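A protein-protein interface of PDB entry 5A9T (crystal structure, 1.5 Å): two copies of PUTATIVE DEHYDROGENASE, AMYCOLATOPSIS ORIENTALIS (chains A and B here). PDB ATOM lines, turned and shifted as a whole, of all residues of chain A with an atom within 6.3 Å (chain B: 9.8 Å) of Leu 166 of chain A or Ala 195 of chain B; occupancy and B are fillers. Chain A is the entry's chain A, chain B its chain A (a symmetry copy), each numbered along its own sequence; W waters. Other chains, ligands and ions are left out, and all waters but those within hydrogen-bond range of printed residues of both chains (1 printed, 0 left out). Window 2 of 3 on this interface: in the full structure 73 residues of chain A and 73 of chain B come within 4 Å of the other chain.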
ATOM      1  N   PRO A  99       7.963   4.271 -36.592  1.00  0.00           N
ATOM      2  CA  PRO A  99       6.669   3.668 -36.677  1.00  0.00           C
ATOM      3  C   PRO A  99       6.005   3.840 -38.037  1.00  0.00           C
ATOM      4  O   PRO A  99       5.418   2.886 -38.585  1.00  0.00           O
ATOM      5  CB  PRO A  99       5.829   4.334 -35.563  1.00  0.00           C
ATOM      6  CG  PRO A  99       6.866   4.714 -34.586  1.00  0.00           C
ATOM      7  CD  PRO A  99       8.056   5.123 -35.339  1.00  0.00           C
ATOM      8  N   ALA A 102       7.521   1.262 -40.441  1.00  0.00           N
ATOM      9  CA  ALA A 102       6.838  -0.055 -40.172  1.00  0.00           C
ATOM     10  C   ALA A 102       5.491  -0.175 -40.795  1.00  0.00           C
ATOM     11  O   ALA A 102       5.207  -1.237 -41.389  1.00  0.00           O
ATOM     12  CB  ALA A 102       6.749  -0.350 -38.650  1.00  0.00           C
ATOM     13  N   ASN A 103       4.612   0.817 -40.647  1.00  0.00           N
ATOM     14  CA  ASN A 103       3.299   0.801 -41.229  1.00  0.00           C
ATOM     15  C   ASN A 103       3.333   0.753 -42.746  1.00  0.00           C
ATOM     16  O   ASN A 103       2.454   0.071 -43.364  1.00  0.00           O
ATOM     17  CB  ASN A 103       2.582   2.044 -40.747  1.00  0.00           C
ATOM     18  CG  ASN A 103       1.691   1.686 -39.639  1.00  0.00           C
ATOM     19  OD1 ASN A 103       0.618   1.174 -39.888  1.00  0.00           O
ATOM     20  ND2 ASN A 103       2.205   1.661 -38.466  1.00  0.00           N
ATOM     21  N   LEU A 136      10.663  -7.509 -29.140  1.00  0.00           N
ATOM     22  CA  LEU A 136       9.294  -7.012 -29.132  1.00  0.00           C
ATOM     23  C   LEU A 136       8.727  -7.034 -30.566  1.00  0.00           C
ATOM     24  O   LEU A 136       9.443  -6.636 -31.487  1.00  0.00           O
ATOM     25  CB  LEU A 136       9.191  -5.606 -28.596  1.00  0.00           C
ATOM     26  CG  LEU A 136       9.848  -5.407 -27.210  1.00  0.00           C
ATOM     27  CD1 LEU A 136       9.685  -3.944 -26.812  1.00  0.00           C
ATOM     28  CD2 LEU A 136       9.262  -6.291 -26.144  1.00  0.00           C
ATOM     29  N   TYR A 137       7.544  -7.556 -30.743  1.00  0.00           N
ATOM     30  CA  TYR A 137       6.924  -7.668 -32.032  1.00  0.00           C
ATOM     31  C   TYR A 137       5.554  -6.973 -32.123  1.00  0.00           C
ATOM     32  O   TYR A 137       4.805  -6.905 -31.169  1.00  0.00           O
ATOM     33  CB  TYR A 137       6.731  -9.142 -32.427  1.00  0.00           C
ATOM     34  CG  TYR A 137       7.983  -9.932 -32.573  1.00  0.00           C
ATOM     35  CD1 TYR A 137       8.691  -9.980 -33.733  1.00  0.00           C
ATOM     36  CD2 TYR A 137       8.530 -10.678 -31.488  1.00  0.00           C
ATOM     37  CE1 TYR A 137       9.879 -10.667 -33.846  1.00  0.00           C
ATOM     38  CE2 TYR A 137       9.662 -11.390 -31.598  1.00  0.00           C
ATOM     39  CZ  TYR A 137      10.358 -11.403 -32.773  1.00  0.00           C
ATOM     40  OH  TYR A 137      11.507 -12.107 -32.944  1.00  0.00           O
ATOM     41  N   SER A 138       5.246  -6.554 -33.323  1.00  0.00           N
ATOM     42  CA  SER A 138       3.964  -5.959 -33.636  1.00  0.00           C
ATOM     43  C   SER A 138       3.591  -6.241 -35.094  1.00  0.00           C
ATOM     44  O   SER A 138       4.421  -6.211 -35.986  1.00  0.00           O
ATOM     45  CB  SER A 138       3.958  -4.420 -33.217  1.00  0.00           C
ATOM     46  OG  SER A 138       4.871  -3.719 -33.908  1.00  0.00           O
ATOM     47  N   LEU A 160       3.108  -7.258 -29.019  1.00  0.00           N
ATOM     48  CA  LEU A 160       2.561  -6.029 -28.383  1.00  0.00           C
ATOM     49  C   LEU A 160       1.194  -5.750 -28.856  1.00  0.00           C
ATOM     50  O   LEU A 160       0.422  -5.115 -28.150  1.00  0.00           O
ATOM     51  CB  LEU A 160       3.409  -4.845 -28.673  1.00  0.00           C
ATOM     52  CG  LEU A 160       4.853  -4.946 -28.153  1.00  0.00           C
ATOM     53  CD1 LEU A 160       5.649  -3.838 -28.747  1.00  0.00           C
ATOM     54  CD2 LEU A 160       4.908  -4.955 -26.640  1.00  0.00           C
ATOM     55  N   GLY A 161       0.850  -6.129 -30.070  1.00  0.00           N
ATOM     56  CA  GLY A 161      -0.394  -5.718 -30.749  1.00  0.00           C
ATOM     57  C   GLY A 161      -0.294  -5.786 -32.250  1.00  0.00           C
ATOM     58  O   GLY A 161       0.767  -6.051 -32.813  1.00  0.00           O
ATOM     59  N   THR A 162      -1.438  -5.533 -32.937  1.00  0.00           N
ATOM     60  CA  THR A 162      -1.491  -5.554 -34.384  1.00  0.00           C
ATOM     61  C   THR A 162      -0.985  -4.430 -35.186  1.00  0.00           C
ATOM     62  O   THR A 162      -0.627  -4.508 -36.342  1.00  0.00           O
ATOM     63  CB  THR A 162      -2.918  -6.020 -34.831  1.00  0.00           C
ATOM     64  OG1 THR A 162      -3.806  -5.030 -34.319  1.00  0.00           O
ATOM     65  CG2 THR A 162      -3.293  -7.320 -34.197  1.00  0.00           C
ATOM     66  N   GLU A 163      -0.876  -3.199 -34.537  1.00  0.00           N
ATOM     67  CA  GLU A 163      -0.387  -2.054 -35.223  1.00  0.00           C
ATOM     68  C   GLU A 163       1.085  -2.214 -35.529  1.00  0.00           C
ATOM     69  O   GLU A 163       1.910  -2.427 -34.600  1.00  0.00           O
ATOM     70  CB  GLU A 163      -0.619  -0.788 -34.359  1.00  0.00           C
ATOM     71  CG  GLU A 163      -0.211   0.542 -35.034  1.00  0.00           C
ATOM     72  CD  GLU A 163      -0.278   1.755 -34.082  1.00  0.00           C
ATOM     73  OE1 GLU A 163      -1.016   1.740 -33.064  1.00  0.00           O
ATOM     74  OE2 GLU A 163       0.411   2.741 -34.339  1.00  0.00           O
ATOM     75  N   ALA A 164       1.492  -2.073 -36.762  1.00  0.00           N
ATOM     76  CA  ALA A 164       2.789  -2.432 -37.175  1.00  0.00           C
ATOM     77  C   ALA A 164       3.937  -1.626 -36.440  1.00  0.00           C
ATOM     78  O   ALA A 164       5.010  -2.148 -36.147  1.00  0.00           O
ATOM     79  CB  ALA A 164       2.952  -2.337 -38.689  1.00  0.00           C
ATOM     80  N   GLY A 165       3.653  -0.353 -36.168  1.00  0.00           N
ATOM     81  CA  GLY A 165       4.666   0.523 -35.573  1.00  0.00           C
ATOM     82  C   GLY A 165       4.810   0.368 -34.044  1.00  0.00           C
ATOM     83  O   GLY A 165       5.661   1.125 -33.504  1.00  0.00           O
ATOM     84  N   LEU A 166       4.086  -0.437 -33.327  1.00  0.00           N
ATOM     85  CA  LEU A 166       4.133  -0.508 -31.831  1.00  0.00           C
ATOM     86  C   LEU A 166       5.512  -0.962 -31.333  1.00  0.00           C
ATOM     87  O   LEU A 166       6.068  -0.392 -30.369  1.00  0.00           O
ATOM     88  CB  LEU A 166       3.098  -1.347 -31.164  1.00  0.00           C
ATOM     89  CG  LEU A 166       1.674  -0.895 -31.278  1.00  0.00           C
ATOM     90  CD1 LEU A 166       0.810  -2.046 -30.885  1.00  0.00           C
ATOM     91  CD2 LEU A 166       1.423   0.294 -30.298  1.00  0.00           C
ATOM     92  N   ALA A 167       6.161  -1.942 -32.007  1.00  0.00           N
ATOM     93  CA  ALA A 167       7.480  -2.331 -31.501  1.00  0.00           C
ATOM     94  C   ALA A 167       8.488  -1.296 -31.624  1.00  0.00           C
ATOM     95  O   ALA A 167       9.240  -1.082 -30.597  1.00  0.00           O
ATOM     96  CB  ALA A 167       7.939  -3.624 -32.268  1.00  0.00           C
ATOM     97  N   VAL A 168       8.607  -0.555 -32.714  1.00  0.00           N
ATOM     98  CA  VAL A 168       9.605   0.543 -32.872  1.00  0.00           C
ATOM     99  C   VAL A 168       9.232   1.612 -31.854  1.00  0.00           C
ATOM    100  O   VAL A 168      10.130   2.224 -31.279  1.00  0.00           O
ATOM    101  CB  VAL A 168       9.676   1.233 -34.278  1.00  0.00           C
ATOM    102  CG1 VAL A 168      10.734   2.368 -34.299  1.00  0.00           C
ATOM    103  CG2 VAL A 168      10.092   0.248 -35.331  1.00  0.00           C
ATOM    104  N   LEU A 169       7.944   1.864 -31.664  1.00  0.00           N
ATOM    105  CA  LEU A 169       7.562   2.951 -30.743  1.00  0.00           C
ATOM    106  C   LEU A 169       7.989   2.521 -29.315  1.00  0.00           C
ATOM    107  O   LEU A 169       8.511   3.387 -28.564  1.00  0.00           O
ATOM    108  CB  LEU A 169       6.106   3.202 -30.822  1.00  0.00           C
ATOM    109  CG  LEU A 169       5.523   4.300 -29.948  1.00  0.00           C
ATOM    110  CD1 LEU A 169       6.180   5.623 -30.246  1.00  0.00           C
ATOM    111  CD2 LEU A 169       4.027   4.374 -30.119  1.00  0.00           C
ATOM    112  N   TYR A 170       7.718   1.282 -28.899  1.00  0.00           N
ATOM    113  CA  TYR A 170       8.166   0.845 -27.583  1.00  0.00           C
ATOM    114  C   TYR A 170       9.623   0.934 -27.428  1.00  0.00           C
ATOM    115  O   TYR A 170      10.192   1.343 -26.382  1.00  0.00           O
ATOM    116  CB  TYR A 170       7.703  -0.603 -27.309  1.00  0.00           C
ATOM    117  CG  TYR A 170       6.444  -0.789 -26.479  1.00  0.00           C
ATOM    118  CD1 TYR A 170       5.197  -0.547 -26.979  1.00  0.00           C
ATOM    119  CD2 TYR A 170       6.599  -1.196 -25.183  1.00  0.00           C
ATOM    120  CE1 TYR A 170       4.047  -0.816 -26.080  1.00  0.00           C
ATOM    121  CE2 TYR A 170       5.532  -1.414 -24.358  1.00  0.00           C
ATOM    122  CZ  TYR A 170       4.325  -1.251 -24.844  1.00  0.00           C
ATOM    123  OH  TYR A 170       3.350  -1.489 -23.760  1.00  0.00           O
ATOM    124  N   ASN A 171      10.403   0.494 -28.438  1.00  0.00           N
ATOM    125  CA  ASN A 171      11.853   0.572 -28.398  1.00  0.00           C
ATOM    126  C   ASN A 171      12.299   2.036 -28.168  1.00  0.00           C
ATOM    127  O   ASN A 171      13.119   2.287 -27.309  1.00  0.00           O
ATOM    128  CB  ASN A 171      12.480   0.024 -29.658  1.00  0.00           C
ATOM    129  CG  ASN A 171      13.967  -0.141 -29.530  1.00  0.00           C
ATOM    130  OD1 ASN A 171      14.550  -0.372 -28.508  1.00  0.00           O
ATOM    131  ND2 ASN A 171      14.600   0.029 -30.601  1.00  0.00           N
ATOM    132  N   ALA B 188       8.703   8.293 -21.867  1.00  0.00           N
ATOM    133  CA  ALA B 188       8.382   7.026 -22.465  1.00  0.00           C
ATOM    134  C   ALA B 188       6.878   6.752 -22.491  1.00  0.00           C
ATOM    135  O   ALA B 188       6.317   6.281 -23.490  1.00  0.00           O
ATOM    136  CB  ALA B 188       9.094   5.948 -21.750  1.00  0.00           C
ATOM    137  N   ALA B 189       6.209   7.020 -21.368  1.00  0.00           N
ATOM    138  CA  ALA B 189       4.778   6.855 -21.246  1.00  0.00           C
ATOM    139  C   ALA B 189       4.046   7.774 -22.206  1.00  0.00           C
ATOM    140  O   ALA B 189       3.055   7.384 -22.803  1.00  0.00           O
ATOM    141  CB  ALA B 189       4.343   6.987 -19.793  1.00  0.00           C
ATOM    142  N   ALA B 190       4.500   8.985 -22.336  1.00  0.00           N
ATOM    143  CA  ALA B 190       3.899   9.876 -23.341  1.00  0.00           C
ATOM    144  C   ALA B 190       4.078   9.326 -24.756  1.00  0.00           C
ATOM    145  O   ALA B 190       3.118   9.436 -25.552  1.00  0.00           O
ATOM    146  CB  ALA B 190       4.472  11.242 -23.169  1.00  0.00           C
ATOM    147  N   LEU B 191       5.231   8.791 -25.072  1.00  0.00           N
ATOM    148  CA  LEU B 191       5.467   8.191 -26.400  1.00  0.00           C
ATOM    149  C   LEU B 191       4.560   7.065 -26.659  1.00  0.00           C
ATOM    150  O   LEU B 191       3.860   7.060 -27.673  1.00  0.00           O
ATOM    151  CB  LEU B 191       6.922   7.761 -26.569  1.00  0.00           C
ATOM    152  CG  LEU B 191       7.915   8.839 -26.850  1.00  0.00           C
ATOM    153  CD1 LEU B 191       9.346   8.379 -26.626  1.00  0.00           C
ATOM    154  CD2 LEU B 191       7.687   9.290 -28.303  1.00  0.00           C
ATOM    155  N   VAL B 192       4.484   6.066 -25.780  1.00  0.00           N
ATOM    156  CA  VAL B 192       3.530   4.926 -26.093  1.00  0.00           C
ATOM    157  C   VAL B 192       2.093   5.385 -25.973  1.00  0.00           C
ATOM    158  O   VAL B 192       1.196   4.876 -26.653  1.00  0.00           O
ATOM    159  CB  VAL B 192       3.824   3.640 -25.301  1.00  0.00           C
ATOM    160  CG1 VAL B 192       5.210   3.184 -25.591  1.00  0.00           C
ATOM    161  CG2 VAL B 192       3.610   3.832 -23.764  1.00  0.00           C
ATOM    162  N   GLY B 193       1.822   6.388 -25.151  1.00  0.00           N
ATOM    163  CA  GLY B 193       0.496   6.937 -24.988  1.00  0.00           C
ATOM    164  C   GLY B 193       0.014   7.575 -26.251  1.00  0.00           C
ATOM    165  O   GLY B 193      -1.210   7.610 -26.456  1.00  0.00           O
ATOM    166  N   SER B 194       0.912   8.011 -27.145  1.00  0.00           N
ATOM    167  CA  SER B 194       0.476   8.602 -28.445  1.00  0.00           C
ATOM    168  C   SER B 194      -0.128   7.532 -29.323  1.00  0.00           C
ATOM    169  O   SER B 194      -0.803   7.908 -30.336  1.00  0.00           O
ATOM    170  CB  SER B 194       1.658   9.335 -29.097  1.00  0.00           C
ATOM    171  OG  SER B 194       2.614   8.461 -29.561  1.00  0.00           O
ATOM    172  N   ALA B 195       0.100   6.280 -29.041  1.00  0.00           N
ATOM    173  CA  ALA B 195      -0.488   5.162 -29.730  1.00  0.00           C
ATOM    174  C   ALA B 195      -1.588   4.496 -28.895  1.00  0.00           C
ATOM    175  O   ALA B 195      -2.072   3.403 -29.281  1.00  0.00           O
ATOM    176  CB  ALA B 195       0.594   4.193 -30.199  1.00  0.00           C
ATOM    177  N   GLY B 196      -2.063   5.159 -27.843  1.00  0.00           N
ATOM    178  CA  GLY B 196      -3.174   4.663 -27.066  1.00  0.00           C
ATOM    179  C   GLY B 196      -2.810   3.713 -25.977  1.00  0.00           C
ATOM    180  O   GLY B 196      -3.718   3.205 -25.324  1.00  0.00           O
ATOM    181  N   VAL B 197      -1.513   3.518 -25.645  1.00  0.00           N
ATOM    182  CA  VAL B 197      -1.102   2.584 -24.619  1.00  0.00           C
ATOM    183  C   VAL B 197      -1.167   3.234 -23.271  1.00  0.00           C
ATOM    184  O   VAL B 197      -0.487   4.235 -23.017  1.00  0.00           O
ATOM    185  CB  VAL B 197       0.347   2.074 -24.857  1.00  0.00           C
ATOM    186  CG1 VAL B 197       0.774   1.152 -23.716  1.00  0.00           C
ATOM    187  CG2 VAL B 197       0.514   1.438 -26.271  1.00  0.00           C
ATOM    188  N   PRO B 198      -2.004   2.744 -22.342  1.00  0.00           N
ATOM    189  CA  PRO B 198      -1.984   3.342 -21.006  1.00  0.00           C
ATOM    190  C   PRO B 198      -0.721   3.137 -20.233  1.00  0.00           C
ATOM    191  O   PRO B 198      -0.029   2.148 -20.410  1.00  0.00           O
ATOM    192  CB  PRO B 198      -3.124   2.601 -20.298  1.00  0.00           C
ATOM    193  CG  PRO B 198      -3.907   1.899 -21.348  1.00  0.00           C
ATOM    194  CD  PRO B 198      -2.949   1.628 -22.474  1.00  0.00           C
ATOM    195  N   ALA B 199      -0.415   4.090 -19.347  1.00  0.00           N
ATOM    196  CA  ALA B 199       0.735   3.997 -18.520  1.00  0.00           C
ATOM    197  C   ALA B 199       0.773   2.718 -17.687  1.00  0.00           C
ATOM    198  O   ALA B 199       1.816   2.104 -17.504  1.00  0.00           O
ATOM    199  CB  ALA B 199       0.882   5.213 -17.603  1.00  0.00           C
ATOM    200  N   GLU B 201      -0.480  -0.183 -18.367  1.00  0.00           N
ATOM    201  CA  GLU B 201      -0.072  -1.263 -19.303  1.00  0.00           C
ATOM    202  C   GLU B 201       1.415  -1.257 -19.579  1.00  0.00           C
ATOM    203  O   GLU B 201       2.153  -2.270 -19.481  1.00  0.00           O
ATOM    204  CB  GLU B 201      -0.901  -1.250 -20.568  1.00  0.00           C
ATOM    205  CG  GLU B 201      -0.622  -2.404 -21.471  1.00  0.00           C
ATOM    206  CD  GLU B 201      -1.050  -3.766 -20.908  1.00  0.00           C
ATOM    207  OE1 GLU B 201      -1.742  -3.870 -19.879  1.00  0.00           O
ATOM    208  OE2 GLU B 201      -0.574  -4.798 -21.487  1.00  0.00           O
ATOM    209  N   PHE B 202       1.888  -0.046 -19.850  1.00  0.00           N
ATOM    210  CA  PHE B 202       3.299   0.183 -20.288  1.00  0.00           C
ATOM    211  C   PHE B 202       4.213  -0.287 -19.104  1.00  0.00           C
ATOM    212  O   PHE B 202       5.308  -0.868 -19.320  1.00  0.00           O
ATOM    213  CB  PHE B 202       3.554   1.610 -20.605  1.00  0.00           C
ATOM    214  CG  PHE B 202       4.946   1.953 -21.009  1.00  0.00           C
ATOM    215  CD1 PHE B 202       5.596   1.259 -22.042  1.00  0.00           C
ATOM    216  CD2 PHE B 202       5.643   2.935 -20.368  1.00  0.00           C
ATOM    217  CE1 PHE B 202       6.887   1.615 -22.405  1.00  0.00           C
ATOM    218  CE2 PHE B 202       6.954   3.270 -20.753  1.00  0.00           C
ATOM    219  CZ  PHE B 202       7.554   2.582 -21.754  1.00  0.00           C
ATOM    220  N   LEU B 205       6.059  -3.906 -19.083  1.00  0.00           N
ATOM    221  CA  LEU B 205       7.322  -4.078 -19.704  1.00  0.00           C
ATOM    222  C   LEU B 205       8.378  -3.055 -19.176  1.00  0.00           C
ATOM    223  O   LEU B 205       9.509  -3.424 -18.919  1.00  0.00           O
ATOM    224  CB  LEU B 205       7.214  -3.978 -21.212  1.00  0.00           C
ATOM    225  CG  LEU B 205       6.626  -5.241 -21.839  1.00  0.00           C
ATOM    226  CD1 LEU B 205       6.271  -4.953 -23.257  1.00  0.00           C
ATOM    227  CD2 LEU B 205       7.600  -6.369 -21.844  1.00  0.00           C
ATOM    228  N   THR B 251      11.383  10.549 -33.971  1.00  0.00           N
ATOM    229  CA  THR B 251      10.231   9.765 -33.775  1.00  0.00           C
ATOM    230  C   THR B 251       9.218  10.495 -32.841  1.00  0.00           C
ATOM    231  O   THR B 251       7.998  10.396 -32.992  1.00  0.00           O
ATOM    232  CB  THR B 251      10.583   8.387 -33.190  1.00  0.00           C
ATOM    233  OG1 THR B 251      11.299   7.685 -34.262  1.00  0.00           O
ATOM    234  CG2 THR B 251       9.385   7.587 -32.819  1.00  0.00           C
ATOM    235  N   GLU B 254       7.349  12.920 -34.949  1.00  0.00           N
ATOM    236  CA  GLU B 254       6.368  12.213 -35.820  1.00  0.00           C
ATOM    237  C   GLU B 254       5.147  11.808 -35.002  1.00  0.00           C
ATOM    238  O   GLU B 254       4.017  11.861 -35.491  1.00  0.00           O
ATOM    239  CB  GLU B 254       6.962  11.015 -36.527  1.00  0.00           C
ATOM    240  CG  GLU B 254       8.010  11.348 -37.537  1.00  0.00           C
ATOM    241  N   GLN B 255       5.331  11.489 -33.697  1.00  0.00           N
ATOM    242  CA  GLN B 255       4.233  11.151 -32.855  1.00  0.00           C
ATOM    243  C   GLN B 255       3.490  12.278 -32.159  1.00  0.00           C
ATOM    244  O   GLN B 255       2.496  12.064 -31.439  1.00  0.00           O
ATOM    245  CB  GLN B 255       4.671  10.182 -31.735  1.00  0.00           C
ATOM    246  CG  GLN B 255       5.184   8.841 -32.279  1.00  0.00           C
ATOM    247  CD  GLN B 255       4.167   8.023 -32.992  1.00  0.00           C
ATOM    248  OE1 GLN B 255       4.359   7.723 -34.162  1.00  0.00           O
ATOM    249  NE2 GLN B 255       3.021   7.692 -32.336  1.00  0.00           N
ATOM    250  N   GLY B 256       3.999  13.489 -32.338  1.00  0.00           N
ATOM    251  CA  GLY B 256       3.374  14.654 -31.698  1.00  0.00           C
ATOM    252  C   GLY B 256       3.666  14.748 -30.227  1.00  0.00           C
ATOM    253  O   GLY B 256       2.865  15.301 -29.448  1.00  0.00           O
ATOM    254  N   VAL B 257       4.823  14.212 -29.795  1.00  0.00           N
ATOM    255  CA  VAL B 257       5.211  14.221 -28.431  1.00  0.00           C
ATOM    256  C   VAL B 257       6.362  15.171 -28.194  1.00  0.00           C
ATOM    257  O   VAL B 257       7.262  15.280 -29.057  1.00  0.00           O
ATOM    258  CB  VAL B 257       5.587  12.752 -27.999  1.00  0.00           C
ATOM    259  CG1 VAL B 257       6.280  12.700 -26.643  1.00  0.00           C
ATOM    260  CG2 VAL B 257       4.351  11.881 -28.070  1.00  0.00           C
HETATM  261  O   HOH W   1       3.768  -3.316 -21.391  1.00  0.00           O
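Among the printed residues, merely in contact across the chains: Pro 99 of chain A with Thr 251 of chain B (3.8 Å), Pro 99 of chain A with Gln 255 of chain B (3.9 Å), Leu 160 of chain A with Leu 205 of chain B (3.6 Å), Leu 166 of chain A with Ala 195 of chain B (3.99 Å), Leu 169 of chain A with Leu 191 of chain B (3.6 Å), Leu 169 of chain A with Ala 195 of chain B (3.4 Å), Leu 169 of chain A with Gln 255 of chain B (3.9 Å), Tyr 170 of chain A with Val 192 of chain B (3.98 Å), Tyr 170 of chain A with Val 197 of chain B (3.7 Å), Tyr 170 of chain A with Phe 202 of chain B (3.5 Å) and Tyr 170 of chain A with Leu 205 of chain B (3.8 Å).
No position is printed for both chains.
Hydrophobic or aromatic side chains of chain A within 4 Å of the printed part of chain B: Pro 99, Leu 160, Leu 166, Leu 169 and Tyr 170. Of the 20 printed residues of chain B, 8 touch a printed residue of chain A. Hydrophobic or aromatic side chains of chain B within 4 Å of the printed part of chain A: Val 192, Ala 195, Val 197, Phe 202 and Leu 205. Along chain B the printed residues that touch a printed residue of chain A span positions 191 to 255. Among the printed residues, no Asp or Glu carboxylate lies within 4 Å of a Lys or Arg side-chain nitrogen of the other chain.
Of the printed residues of chain B, Leu 166 of chain A touches Ala 195. Of the printed residues of chain A, Ala 195 of chain B touches Leu 166 and Leu 169. No residue of chain B comes within 4 Å of Gly 161 of chain A. No residue of chain B comes within 4 Å of Ala 167 of chain A. Of the printed residues of chain B, Tyr 170 of chain A touches Val 192 (3.98 Å), Val 197 (3.7 Å), Phe 202 (3.5 Å) and Leu 205 (3.8 Å). Of the printed residues of chain B, Pro 99 of chain A touches Thr 251 (3.8 Å) and Gln 255 (3.9 Å). Of the printed residues of chain A, Val 197 of chain B touches Tyr 170 (3.7 Å). Of the printed residues of chain A, Leu 205 of chain B touches Leu 160 and Tyr 170. Gly 256 of chain B touches none of the printed residues of chain A. The nearest printed residue of chain B that does not touch Leu 166 of chain A is Val 197 of chain B (4.3 Å). The nearest printed residue of chain A that does not touch Ala 195 of chain B is Glu 163 of chain A (4.1 Å).
OG of Ser 194 of chain B sits at hydrogen-bond distance from NE2 of Gln 255 of chain B, at 2.9 Å. The side-chain hydroxyl of Ser 138 of chain A is in hydrogen-bond range of the backbone NH of Leu 166 of chain A, 3.4 Å away. The side-chain hydroxyl (OG) of Ser 194 of chain B sits at hydrogen-bond distance from the backbone carbonyl oxygen (O) of Leu 191 of chain B (2.7 Å). O of Val 192 of chain B sits at hydrogen-bond distance from N of Val 197 of chain B, 3.2 Å away. The backbone carbonyl oxygen of Tyr 137 of chain A sits at hydrogen-bond distance from the backbone NH of Leu 160 of chain A (2.8 Å). ND2 of Asn 103 of chain A is in hydrogen-bond range of O of Pro 99 of chain A (3.4 Å).
Water W1 lies within hydrogen-bond range of the backbone carbonyl oxygen (O) of Glu 201 of chain B, the side-chain hydroxyl (OH) of Tyr 170 of chain A and the backbone NH (N) of Leu 205 of chain B.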
